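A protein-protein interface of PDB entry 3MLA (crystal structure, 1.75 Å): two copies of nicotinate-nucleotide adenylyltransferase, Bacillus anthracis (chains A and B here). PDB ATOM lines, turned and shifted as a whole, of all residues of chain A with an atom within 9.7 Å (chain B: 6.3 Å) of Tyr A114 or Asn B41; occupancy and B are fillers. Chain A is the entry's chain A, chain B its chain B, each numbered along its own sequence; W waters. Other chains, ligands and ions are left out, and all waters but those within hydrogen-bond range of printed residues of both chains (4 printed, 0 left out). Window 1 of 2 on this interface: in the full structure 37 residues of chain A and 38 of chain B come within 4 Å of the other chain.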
ATOM      1  N   ILE A 107     -21.345  19.688 -13.990  1.00  0.00           N
ATOM      2  CA  ILE A 107     -20.864  18.846 -12.907  1.00  0.00           C
ATOM      3  C   ILE A 107     -19.433  19.243 -12.513  1.00  0.00           C
ATOM      4  O   ILE A 107     -18.685  19.808 -13.314  1.00  0.00           O
ATOM      5  CB  ILE A 107     -20.891  17.354 -13.300  1.00  0.00           C
ATOM      6  CG1 ILE A 107     -20.042  17.119 -14.547  1.00  0.00           C
ATOM      7  CG2 ILE A 107     -22.327  16.895 -13.572  1.00  0.00           C
ATOM      8  CD1 ILE A 107     -19.981  15.653 -14.990  1.00  0.00           C
ATOM      9  N   GLY A 108     -19.061  18.944 -11.274  1.00  0.00           N
ATOM     10  CA  GLY A 108     -17.717  19.219 -10.802  1.00  0.00           C
ATOM     11  C   GLY A 108     -16.715  18.249 -11.398  1.00  0.00           C
ATOM     12  O   GLY A 108     -17.046  17.098 -11.715  1.00  0.00           O
ATOM     13  N   GLY A 109     -15.479  18.712 -11.532  1.00  0.00           N
ATOM     14  CA  GLY A 109     -14.405  17.915 -12.095  1.00  0.00           C
ATOM     15  C   GLY A 109     -14.214  16.584 -11.403  1.00  0.00           C
ATOM     16  O   GLY A 109     -13.909  15.591 -12.054  1.00  0.00           O
ATOM     17  N   ASP A 110     -14.405  16.563 -10.087  1.00  0.00           N
ATOM     18  CA  ASP A 110     -14.308  15.330  -9.292  1.00  0.00           C
ATOM     19  C   ASP A 110     -15.472  14.350  -9.520  1.00  0.00           C
ATOM     20  O   ASP A 110     -15.379  13.169  -9.197  1.00  0.00           O
ATOM     21  CB  ASP A 110     -14.241  15.669  -7.795  1.00  0.00           C
ATOM     22  CG  ASP A 110     -13.088  16.605  -7.449  1.00  0.00           C
ATOM     23  OD1 ASP A 110     -12.521  17.237  -8.369  1.00  0.00           O
ATOM     24  OD2 ASP A 110     -12.758  16.711  -6.246  1.00  0.00           O
ATOM     25  N   MET A 111     -16.588  14.849 -10.030  1.00  0.00           N
ATOM     26  CA  MET A 111     -17.714  13.992 -10.351  1.00  0.00           C
ATOM     27  C   MET A 111     -17.341  13.087 -11.521  1.00  0.00           C
ATOM     28  O   MET A 111     -17.838  11.973 -11.643  1.00  0.00           O
ATOM     29  CB  MET A 111     -18.895  14.853 -10.789  1.00  0.00           C
ATOM     30  CG  MET A 111     -20.032  14.104 -11.415  1.00  0.00           C
ATOM     31  SD  MET A 111     -21.001  13.201 -10.202  1.00  0.00           S
ATOM     32  CE  MET A 111     -20.231  11.589 -10.266  1.00  0.00           C
ATOM     33  N   VAL A 112     -16.482  13.581 -12.402  1.00  0.00           N
ATOM     34  CA  VAL A 112     -16.406  13.008 -13.748  1.00  0.00           C
ATOM     35  C   VAL A 112     -16.049  11.512 -13.793  1.00  0.00           C
ATOM     36  O   VAL A 112     -16.647  10.746 -14.554  1.00  0.00           O
ATOM     37  CB  VAL A 112     -15.478  13.854 -14.654  1.00  0.00           C
ATOM     38  CG1 VAL A 112     -15.161  13.124 -15.956  1.00  0.00           C
ATOM     39  CG2 VAL A 112     -16.100  15.220 -14.914  1.00  0.00           C
ATOM     40  N   GLU A 113     -15.089  11.082 -12.978  1.00  0.00           N
ATOM     41  CA  GLU A 113     -14.668   9.691 -13.075  1.00  0.00           C
ATOM     42  C   GLU A 113     -15.758   8.744 -12.610  1.00  0.00           C
ATOM     43  O   GLU A 113     -15.692   7.563 -12.903  1.00  0.00           O
ATOM     44  CB  GLU A 113     -13.372   9.417 -12.300  1.00  0.00           C
ATOM     45  CG  GLU A 113     -13.559   9.387 -10.802  1.00  0.00           C
ATOM     46  CD  GLU A 113     -12.250   9.257 -10.050  1.00  0.00           C
ATOM     47  OE1 GLU A 113     -11.698  10.295  -9.644  1.00  0.00           O
ATOM     48  OE2 GLU A 113     -11.773   8.125  -9.852  1.00  0.00           O
ATOM     49  N   TYR A 114     -16.755   9.271 -11.888  1.00  0.00           N
ATOM     50  CA  TYR A 114     -17.839   8.430 -11.371  1.00  0.00           C
ATOM     51  C   TYR A 114     -19.132   8.417 -12.200  1.00  0.00           C
ATOM     52  O   TYR A 114     -20.077   7.694 -11.865  1.00  0.00           O
ATOM     53  CB  TYR A 114     -18.144   8.808  -9.914  1.00  0.00           C
ATOM     54  CG  TYR A 114     -16.947   8.610  -9.013  1.00  0.00           C
ATOM     55  CD1 TYR A 114     -16.252   9.695  -8.484  1.00  0.00           C
ATOM     56  CD2 TYR A 114     -16.501   7.336  -8.708  1.00  0.00           C
ATOM     57  CE1 TYR A 114     -15.154   9.498  -7.667  1.00  0.00           C
ATOM     58  CE2 TYR A 114     -15.413   7.133  -7.898  1.00  0.00           C
ATOM     59  CZ  TYR A 114     -14.744   8.211  -7.378  1.00  0.00           C
ATOM     60  OH  TYR A 114     -13.654   7.982  -6.570  1.00  0.00           O
ATOM     61  N   LEU A 115     -19.171   9.184 -13.287  1.00  0.00           N
ATOM     62  CA  LEU A 115     -20.320   9.148 -14.212  1.00  0.00           C
ATOM     63  C   LEU A 115     -20.848   7.761 -14.602  1.00  0.00           C
ATOM     64  O   LEU A 115     -22.077   7.579 -14.727  1.00  0.00           O
ATOM     65  CB  LEU A 115     -20.039   9.964 -15.481  1.00  0.00           C
ATOM     66  CG  LEU A 115     -20.063  11.480 -15.308  1.00  0.00           C
ATOM     67  CD1 LEU A 115     -19.583  12.144 -16.595  1.00  0.00           C
ATOM     68  CD2 LEU A 115     -21.468  11.965 -14.908  1.00  0.00           C
ATOM     69  N   PRO A 116     -19.949   6.785 -14.828  1.00  0.00           N
ATOM     70  CA  PRO A 116     -20.458   5.471 -15.237  1.00  0.00           C
ATOM     71  C   PRO A 116     -21.342   4.816 -14.180  1.00  0.00           C
ATOM     72  O   PRO A 116     -22.028   3.847 -14.492  1.00  0.00           O
ATOM     73  CB  PRO A 116     -19.182   4.648 -15.457  1.00  0.00           C
ATOM     74  CG  PRO A 116     -18.124   5.693 -15.794  1.00  0.00           C
ATOM     75  CD  PRO A 116     -18.476   6.861 -14.910  1.00  0.00           C
ATOM     76  N   LYS A 117     -21.328   5.345 -12.956  1.00  0.00           N
ATOM     77  CA  LYS A 117     -22.119   4.788 -11.855  1.00  0.00           C
ATOM     78  C   LYS A 117     -23.465   5.481 -11.680  1.00  0.00           C
ATOM     79  O   LYS A 117     -24.246   5.088 -10.806  1.00  0.00           O
ATOM     80  CB  LYS A 117     -21.336   4.879 -10.539  1.00  0.00           C
ATOM     81  CG  LYS A 117     -20.078   4.038 -10.507  1.00  0.00           C
ATOM     82  CD  LYS A 117     -19.268   4.326  -9.250  1.00  0.00           C
ATOM     83  CE  LYS A 117     -18.149   3.307  -9.079  1.00  0.00           C
ATOM     84  NZ  LYS A 117     -18.684   1.938  -9.003  1.00  0.00           N
ATOM     85  N   TRP A 118     -23.731   6.519 -12.476  1.00  0.00           N
ATOM     86  CA  TRP A 118     -25.026   7.202 -12.405  1.00  0.00           C
ATOM     87  C   TRP A 118     -26.110   6.315 -12.979  1.00  0.00           C
ATOM     88  O   TRP A 118     -25.884   5.590 -13.953  1.00  0.00           O
ATOM     89  CB  TRP A 118     -24.999   8.510 -13.201  1.00  0.00           C
ATOM     90  CG  TRP A 118     -24.237   9.649 -12.548  1.00  0.00           C
ATOM     91  CD1 TRP A 118     -23.138   9.553 -11.739  1.00  0.00           C
ATOM     92  CD2 TRP A 118     -24.493  11.054 -12.704  1.00  0.00           C
ATOM     93  NE1 TRP A 118     -22.717  10.797 -11.366  1.00  0.00           N
ATOM     94  CE2 TRP A 118     -23.531  11.740 -11.944  1.00  0.00           C
ATOM     95  CE3 TRP A 118     -25.452  11.793 -13.405  1.00  0.00           C
ATOM     96  CZ2 TRP A 118     -23.493  13.133 -11.862  1.00  0.00           C
ATOM     97  CZ3 TRP A 118     -25.421  13.175 -13.322  1.00  0.00           C
ATOM     98  CH2 TRP A 118     -24.446  13.834 -12.555  1.00  0.00           C
ATOM     99  N   TYR A 119     -27.295   6.381 -12.378  1.00  0.00           N
ATOM    100  CA  TYR A 119     -28.438   5.633 -12.860  1.00  0.00           C
ATOM    101  C   TYR A 119     -28.774   6.021 -14.313  1.00  0.00           C
ATOM    102  O   TYR A 119     -28.898   7.208 -14.634  1.00  0.00           O
ATOM    103  CB  TYR A 119     -29.625   5.891 -11.924  1.00  0.00           C
ATOM    104  CG  TYR A 119     -30.927   5.345 -12.442  1.00  0.00           C
ATOM    105  CD1 TYR A 119     -31.177   3.983 -12.434  1.00  0.00           C
ATOM    106  CD2 TYR A 119     -31.907   6.194 -12.937  1.00  0.00           C
ATOM    107  CE1 TYR A 119     -32.376   3.474 -12.907  1.00  0.00           C
ATOM    108  CE2 TYR A 119     -33.112   5.688 -13.422  1.00  0.00           C
ATOM    109  CZ  TYR A 119     -33.333   4.331 -13.402  1.00  0.00           C
ATOM    110  OH  TYR A 119     -34.518   3.809 -13.878  1.00  0.00           O
ATOM    111  N   ILE A 121     -27.006   6.156 -16.959  1.00  0.00           N
ATOM    112  CA  ILE A 121     -26.054   7.110 -17.532  1.00  0.00           C
ATOM    113  C   ILE A 121     -26.109   7.111 -19.063  1.00  0.00           C
ATOM    114  O   ILE A 121     -26.099   8.173 -19.683  1.00  0.00           O
ATOM    115  CB  ILE A 121     -24.591   6.888 -17.027  1.00  0.00           C
ATOM    116  CG1 ILE A 121     -23.622   7.914 -17.645  1.00  0.00           C
ATOM    117  CG2 ILE A 121     -24.113   5.487 -17.341  1.00  0.00           C
ATOM    118  CD1 ILE A 121     -23.849   9.347 -17.210  1.00  0.00           C
ATOM    119  N   LEU A 124     -29.092   8.949 -20.196  1.00  0.00           N
ATOM    120  CA  LEU A 124     -28.935  10.354 -19.824  1.00  0.00           C
ATOM    121  C   LEU A 124     -28.021  11.105 -20.805  1.00  0.00           C
ATOM    122  O   LEU A 124     -28.261  12.274 -21.102  1.00  0.00           O
ATOM    123  CB  LEU A 124     -28.428  10.468 -18.376  1.00  0.00           C
ATOM    124  CG  LEU A 124     -28.089  11.830 -17.783  1.00  0.00           C
ATOM    125  CD1 LEU A 124     -29.273  12.801 -17.850  1.00  0.00           C
ATOM    126  CD2 LEU A 124     -27.642  11.622 -16.332  1.00  0.00           C
ATOM    127  N   PHE A 130     -23.054  17.021 -20.912  1.00  0.00           N
ATOM    128  CA  PHE A 130     -22.385  17.316 -19.644  1.00  0.00           C
ATOM    129  C   PHE A 130     -21.353  18.412 -19.817  1.00  0.00           C
ATOM    130  O   PHE A 130     -20.649  18.469 -20.831  1.00  0.00           O
ATOM    131  CB  PHE A 130     -21.714  16.075 -19.042  1.00  0.00           C
ATOM    132  CG  PHE A 130     -22.679  15.125 -18.411  1.00  0.00           C
ATOM    133  CD1 PHE A 130     -23.012  13.931 -19.038  1.00  0.00           C
ATOM    134  CD2 PHE A 130     -23.296  15.446 -17.209  1.00  0.00           C
ATOM    135  CE1 PHE A 130     -23.915  13.055 -18.449  1.00  0.00           C
ATOM    136  CE2 PHE A 130     -24.202  14.585 -16.629  1.00  0.00           C
ATOM    137  CZ  PHE A 130     -24.517  13.392 -17.248  1.00  0.00           C
ATOM    138  N   ARG A 141     -10.830  13.443 -17.630  1.00  0.00           N
ATOM    139  CA  ARG A 141     -10.661  12.196 -18.354  1.00  0.00           C
ATOM    140  C   ARG A 141     -11.894  11.331 -18.156  1.00  0.00           C
ATOM    141  O   ARG A 141     -12.233  10.965 -17.035  1.00  0.00           O
ATOM    142  CB  ARG A 141      -9.387  11.488 -17.883  1.00  0.00           C
ATOM    143  CG  ARG A 141      -8.958  10.320 -18.738  1.00  0.00           C
ATOM    144  CD  ARG A 141      -7.512   9.992 -18.438  1.00  0.00           C
ATOM    145  NE  ARG A 141      -7.015   8.809 -19.134  1.00  0.00           N
ATOM    146  CZ  ARG A 141      -6.095   8.831 -20.094  1.00  0.00           C
ATOM    147  NH1 ARG A 141      -5.572   9.983 -20.501  1.00  0.00           N
ATOM    148  NH2 ARG A 141      -5.696   7.700 -20.651  1.00  0.00           N
ATOM    149  N   THR A 142     -12.582  11.036 -19.257  1.00  0.00           N
ATOM    150  CA  THR A 142     -13.785  10.227 -19.226  1.00  0.00           C
ATOM    151  C   THR A 142     -14.007   9.651 -20.622  1.00  0.00           C
ATOM    152  O   THR A 142     -13.646  10.293 -21.618  1.00  0.00           O
ATOM    153  CB  THR A 142     -15.032  11.047 -18.817  1.00  0.00           C
ATOM    154  OG1 THR A 142     -16.217  10.294 -19.101  1.00  0.00           O
ATOM    155  CG2 THR A 142     -15.111  12.368 -19.568  1.00  0.00           C
ATOM    156  N   PRO A 143     -14.574   8.440 -20.701  1.00  0.00           N
ATOM    157  CA  PRO A 143     -14.872   7.857 -22.017  1.00  0.00           C
ATOM    158  C   PRO A 143     -16.062   8.552 -22.664  1.00  0.00           C
ATOM    159  O   PRO A 143     -16.313   8.378 -23.871  1.00  0.00           O
ATOM    160  CB  PRO A 143     -15.272   6.420 -21.674  1.00  0.00           C
ATOM    161  CG  PRO A 143     -15.870   6.543 -20.286  1.00  0.00           C
ATOM    162  CD  PRO A 143     -14.964   7.537 -19.601  1.00  0.00           C
ATOM    163  N   TYR A 144     -16.806   9.305 -21.858  1.00  0.00           N
ATOM    164  CA  TYR A 144     -18.000   9.983 -22.345  1.00  0.00           C
ATOM    165  C   TYR A 144     -17.667  11.320 -22.983  1.00  0.00           C
ATOM    166  O   TYR A 144     -16.689  11.982 -22.599  1.00  0.00           O
ATOM    167  CB  TYR A 144     -19.008  10.204 -21.211  1.00  0.00           C
ATOM    168  CG  TYR A 144     -19.441   8.929 -20.516  1.00  0.00           C
ATOM    169  CD1 TYR A 144     -19.500   8.862 -19.134  1.00  0.00           C
ATOM    170  CD2 TYR A 144     -19.774   7.789 -21.243  1.00  0.00           C
ATOM    171  CE1 TYR A 144     -19.897   7.709 -18.492  1.00  0.00           C
ATOM    172  CE2 TYR A 144     -20.171   6.616 -20.603  1.00  0.00           C
ATOM    173  CZ  TYR A 144     -20.229   6.594 -19.215  1.00  0.00           C
ATOM    174  OH  TYR A 144     -20.605   5.446 -18.563  1.00  0.00           O
ATOM    175  N   ILE A 146     -17.899  15.038 -23.174  1.00  0.00           N
ATOM    176  CA  ILE A 146     -18.159  16.055 -22.191  1.00  0.00           C
ATOM    177  C   ILE A 146     -17.579  17.367 -22.700  1.00  0.00           C
ATOM    178  O   ILE A 146     -16.614  17.380 -23.482  1.00  0.00           O
ATOM    179  CB  ILE A 146     -17.559  15.671 -20.814  1.00  0.00           C
ATOM    180  CG1 ILE A 146     -17.918  16.700 -19.749  1.00  0.00           C
ATOM    181  CG2 ILE A 146     -16.050  15.504 -20.918  1.00  0.00           C
ATOM    182  CD1 ILE A 146     -17.406  16.332 -18.365  1.00  0.00           C
ATOM    183  N   GLY B  10     -12.854   3.736  -3.257  1.00  0.00           N
ATOM    184  CA  GLY B  10     -13.030   3.380  -4.651  1.00  0.00           C
ATOM    185  C   GLY B  10     -12.668   4.501  -5.616  1.00  0.00           C
ATOM    186  O   GLY B  10     -12.572   5.659  -5.226  1.00  0.00           O
ATOM    187  N   GLY B  11     -12.456   4.163  -6.880  1.00  0.00           N
ATOM    188  CA  GLY B  11     -12.174   5.197  -7.868  1.00  0.00           C
ATOM    189  C   GLY B  11     -11.502   4.556  -9.056  1.00  0.00           C
ATOM    190  O   GLY B  11     -11.341   3.362  -9.064  1.00  0.00           O
ATOM    191  N   THR B  12     -11.118   5.346 -10.053  1.00  0.00           N
ATOM    192  CA  THR B  12     -10.412   4.780 -11.198  1.00  0.00           C
ATOM    193  C   THR B  12      -8.898   4.714 -10.983  1.00  0.00           C
ATOM    194  O   THR B  12      -8.212   3.985 -11.697  1.00  0.00           O
ATOM    195  CB  THR B  12     -10.687   5.569 -12.500  1.00  0.00           C
ATOM    196  OG1 THR B  12     -10.354   6.950 -12.307  1.00  0.00           O
ATOM    197  CG2 THR B  12     -12.161   5.449 -12.871  1.00  0.00           C
ATOM    198  N   PHE B  13      -8.399   5.492 -10.022  1.00  0.00           N
ATOM    199  CA  PHE B  13      -6.981   5.499  -9.649  1.00  0.00           C
ATOM    200  C   PHE B  13      -6.099   5.661 -10.880  1.00  0.00           C
ATOM    201  O   PHE B  13      -5.346   4.766 -11.243  1.00  0.00           O
ATOM    202  CB  PHE B  13      -6.637   4.233  -8.845  1.00  0.00           C
ATOM    203  CG  PHE B  13      -7.435   4.107  -7.564  1.00  0.00           C
ATOM    204  CD1 PHE B  13      -8.371   3.085  -7.403  1.00  0.00           C
ATOM    205  CD2 PHE B  13      -7.266   5.031  -6.535  1.00  0.00           C
ATOM    206  CE1 PHE B  13      -9.112   2.981  -6.231  1.00  0.00           C
ATOM    207  CE2 PHE B  13      -7.999   4.932  -5.362  1.00  0.00           C
ATOM    208  CZ  PHE B  13      -8.925   3.907  -5.217  1.00  0.00           C
ATOM    209  N   LEU B  39     -10.482  -0.038  -4.230  1.00  0.00           N
ATOM    210  CA  LEU B  39     -11.464  -0.708  -5.070  1.00  0.00           C
ATOM    211  C   LEU B  39     -11.496  -0.066  -6.452  1.00  0.00           C
ATOM    212  O   LEU B  39     -12.255   0.866  -6.696  1.00  0.00           O
ATOM    213  CB  LEU B  39     -12.856  -0.628  -4.418  1.00  0.00           C
ATOM    214  CG  LEU B  39     -13.989  -1.316  -5.198  1.00  0.00           C
ATOM    215  CD1 LEU B  39     -13.982  -2.820  -4.971  1.00  0.00           C
ATOM    216  CD2 LEU B  39     -15.348  -0.722  -4.839  1.00  0.00           C
ATOM    217  N   PRO B  40     -10.642  -0.550  -7.365  1.00  0.00           N
ATOM    218  CA  PRO B  40     -10.590   0.074  -8.690  1.00  0.00           C
ATOM    219  C   PRO B  40     -11.899  -0.118  -9.451  1.00  0.00           C
ATOM    220  O   PRO B  40     -12.452  -1.224  -9.484  1.00  0.00           O
ATOM    221  CB  PRO B  40      -9.443  -0.673  -9.386  1.00  0.00           C
ATOM    222  CG  PRO B  40      -9.301  -1.975  -8.611  1.00  0.00           C
ATOM    223  CD  PRO B  40      -9.628  -1.606  -7.198  1.00  0.00           C
ATOM    224  N   ASN B  41     -12.387   0.965 -10.053  1.00  0.00           N
ATOM    225  CA  ASN B  41     -13.621   0.930 -10.829  1.00  0.00           C
ATOM    226  C   ASN B  41     -13.368   0.481 -12.268  1.00  0.00           C
ATOM    227  O   ASN B  41     -12.272   0.662 -12.811  1.00  0.00           O
ATOM    228  CB  ASN B  41     -14.249   2.321 -10.931  1.00  0.00           C
ATOM    229  CG  ASN B  41     -14.632   2.936  -9.586  1.00  0.00           C
ATOM    230  OD1 ASN B  41     -14.794   4.150  -9.514  1.00  0.00           O
ATOM    231  ND2 ASN B  41     -14.797   2.125  -8.539  1.00  0.00           N
ATOM    232  N   GLN B  42     -14.393  -0.076 -12.902  1.00  0.00           N
ATOM    233  CA  GLN B  42     -14.315  -0.348 -14.337  1.00  0.00           C
ATOM    234  C   GLN B  42     -14.546   0.963 -15.085  1.00  0.00           C
ATOM    235  O   GLN B  42     -15.297   1.821 -14.615  1.00  0.00           O
ATOM    236  CB  GLN B  42     -15.352  -1.397 -14.752  1.00  0.00           C
ATOM    237  CG  GLN B  42     -15.082  -2.030 -16.112  1.00  0.00           C
ATOM    238  CD  GLN B  42     -13.646  -2.523 -16.270  1.00  0.00           C
ATOM    239  OE1 GLN B  42     -12.756  -1.771 -16.691  1.00  0.00           O
ATOM    240  NE2 GLN B  42     -13.416  -3.791 -15.939  1.00  0.00           N
ATOM    241  N   ILE B  43     -13.871   1.135 -16.224  1.00  0.00           N
ATOM    242  CA  ILE B  43     -14.127   2.280 -17.104  1.00  0.00           C
ATOM    243  C   ILE B  43     -14.703   1.761 -18.413  1.00  0.00           C
ATOM    244  O   ILE B  43     -14.063   0.955 -19.099  1.00  0.00           O
ATOM    245  CB  ILE B  43     -12.841   3.063 -17.426  1.00  0.00           C
ATOM    246  CG1 ILE B  43     -12.193   3.607 -16.141  1.00  0.00           C
ATOM    247  CG2 ILE B  43     -13.109   4.217 -18.393  1.00  0.00           C
ATOM    248  CD1 ILE B  43     -10.884   4.324 -16.395  1.00  0.00           C
ATOM    249  N   VAL B  55      -6.994  -1.501 -17.862  1.00  0.00           N
ATOM    250  CA  VAL B  55      -7.165  -2.105 -16.547  1.00  0.00           C
ATOM    251  C   VAL B  55      -5.822  -2.636 -16.052  1.00  0.00           C
ATOM    252  O   VAL B  55      -5.485  -2.516 -14.866  1.00  0.00           O
ATOM    253  CB  VAL B  55      -8.172  -3.272 -16.585  1.00  0.00           C
ATOM    254  CG1 VAL B  55      -8.085  -4.092 -15.304  1.00  0.00           C
ATOM    255  CG2 VAL B  55      -9.579  -2.749 -16.786  1.00  0.00           C
ATOM    256  N   ARG B  58      -3.833   0.315 -14.695  1.00  0.00           N
ATOM    257  CA  ARG B  58      -4.336   0.874 -13.454  1.00  0.00           C
ATOM    258  C   ARG B  58      -4.088  -0.065 -12.286  1.00  0.00           C
ATOM    259  O   ARG B  58      -3.720   0.370 -11.198  1.00  0.00           O
ATOM    260  CB  ARG B  58      -5.806   1.231 -13.607  1.00  0.00           C
ATOM    261  CG  ARG B  58      -5.988   2.320 -14.646  1.00  0.00           C
ATOM    262  CD  ARG B  58      -7.396   2.888 -14.625  1.00  0.00           C
ATOM    263  NE  ARG B  58      -8.358   1.939 -15.171  1.00  0.00           N
ATOM    264  CZ  ARG B  58      -9.399   1.463 -14.496  1.00  0.00           C
ATOM    265  NH1 ARG B  58      -9.614   1.850 -13.240  1.00  0.00           N
ATOM    266  NH2 ARG B  58     -10.227   0.605 -15.074  1.00  0.00           N
ATOM    267  N   GLU B  78     -15.051  -5.099  -8.420  1.00  0.00           N
ATOM    268  CA  GLU B  78     -15.640  -4.405  -9.573  1.00  0.00           C
ATOM    269  C   GLU B  78     -14.976  -4.756 -10.916  1.00  0.00           C
ATOM    270  O   GLU B  78     -15.626  -4.733 -11.955  1.00  0.00           O
ATOM    271  CB  GLU B  78     -15.698  -2.886  -9.363  1.00  0.00           C
ATOM    272  CG  GLU B  78     -16.536  -2.458  -8.163  1.00  0.00           C
ATOM    273  CD  GLU B  78     -17.069  -1.039  -8.278  1.00  0.00           C
ATOM    274  OE1 GLU B  78     -17.988  -0.689  -7.504  1.00  0.00           O
ATOM    275  OE2 GLU B  78     -16.575  -0.259  -9.125  1.00  0.00           O
ATOM    276  N   LEU B  79     -13.683  -5.054 -10.902  1.00  0.00           N
ATOM    277  CA  LEU B  79     -12.999  -5.459 -12.133  1.00  0.00           C
ATOM    278  C   LEU B  79     -13.399  -6.860 -12.586  1.00  0.00           C
ATOM    279  O   LEU B  79     -13.169  -7.241 -13.737  1.00  0.00           O
ATOM    280  CB  LEU B  79     -11.482  -5.378 -11.958  1.00  0.00           C
ATOM    281  CG  LEU B  79     -10.941  -3.987 -11.645  1.00  0.00           C
ATOM    282  CD1 LEU B  79      -9.415  -4.001 -11.565  1.00  0.00           C
ATOM    283  CD2 LEU B  79     -11.416  -2.983 -12.689  1.00  0.00           C
HETATM  284  O   HOH W   1     -16.205   5.121 -11.722  1.00  0.00           O
HETATM  285  O   HOH W   2     -18.106   1.419  -5.666  1.00  0.00           O
HETATM  286  O   HOH W   3     -10.639   7.840  -5.775  1.00  0.00           O
HETATM  287  O   HOH W   4      -9.562   7.615  -8.212  1.00  0.00           O
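N of Gly B11 sits at hydrogen-bond distance from O of Leu B39 (3.3 Å). O of Gly B11 is in hydrogen-bond range of N of Asn B41 (2.8 Å). The backbone carbonyl oxygen (O) of Thr B12 is in hydrogen-bond range of the guanidinium group (NH1) of Arg B58, at 3.0 Å. The side-chain amide nitrogen of Asn B41 is in hydrogen-bond range of the backbone carbonyl oxygen of Leu B39 (3.4 Å). The guanidinium group of Arg B58 lies within hydrogen-bond range of the backbone carbonyl oxygen of Asn B41. ND2 of Asn B41 sits at hydrogen-bond distance from OE2 of Glu B78, at 3.0 Å.
No position is printed for both chains.
Of the printed residues of chain B, Glu A113 touches Gly B11 (3.6 Å) and Thr B12 (2.9 Å). Of chain B, only Gly B10, Gly B11 and Asn B41 come within 4 Å of Tyr A114. Of the printed residues of chain B, Pro A143 touches Ile B43 (3.99 Å). Tyr A144 touches none of the printed residues of chain B. Gly B10 touches just one residue of chain A: Tyr A114. Gly B11 touches just these residues of chain A: Glu A113 (3.6 Å) and Tyr A114 (3.4 Å). No residue of chain A comes within 4 Å of Pro B40. Asn B41 touches just these residues of chain A: Tyr A114 and Lys A117. No residue of chain A comes within 4 Å of Gln B42. Val B55 touches none of the printed residues of chain A. The nearest residue of chain A that does not touch Asn B41 is Glu A113 (4.9 Å). The nearest printed residue of chain B that does not touch Pro A143 is Gln B42 (7.4 Å).
The side-chain carboxylate (OE2) of Glu A113 lies within hydrogen-bond range of the backbone NH (N) of Thr B12 (2.9 Å). The side-chain hydroxyl (OH) of Tyr A114 sits at hydrogen-bond distance from the backbone carbonyl oxygen (O) of Gly B10 (2.9 Å). OE2 of Glu B78 lies within salt-bridge range of NZ of Lys A117 (3.0 Å).
Water W1 bridges the backbone carbonyl oxygen of Glu A113 (2.8 Å) and the side-chain amide oxygen of Asn B41 (2.8 Å). Water W2 lies within hydrogen-bond range of the side-chain carboxylate (OE1) of Glu B78 (2.8 Å) and the side-chain amino group (NZ) of Lys A117 (3.4 Å). Water W4 lies within hydrogen-bond range of the side-chain carboxylate of Glu A113 (2.8 Å), the backbone NH of Phe B13 (3.0 Å) and the backbone NH of Thr B12 (3.3 Å). Water W3 bridges O of Gly B10 (3.0 Å) and OH of Tyr A114 (3.1 Å).
Gly B11 touches Glu A113. Gly B11 touches Tyr A114 (CA to OH, 3.4 Å). CE2 of Tyr A114 touches OD1 of Asn B41, at 3.4 Å. Asn B41 touches Lys A117 (OD1 to CE, 3.5 Å). Pro A143 touches Ile B43.
Hydrophobic or aromatic side chains of chain A within 4 Å of the printed part of chain B: Tyr A114 and Pro A143. Hydrophobic or aromatic side chains of chain B within 4 Å of the printed part of chain A: Ile B43. Among the printed residues, 8 pairs touch across the chains.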
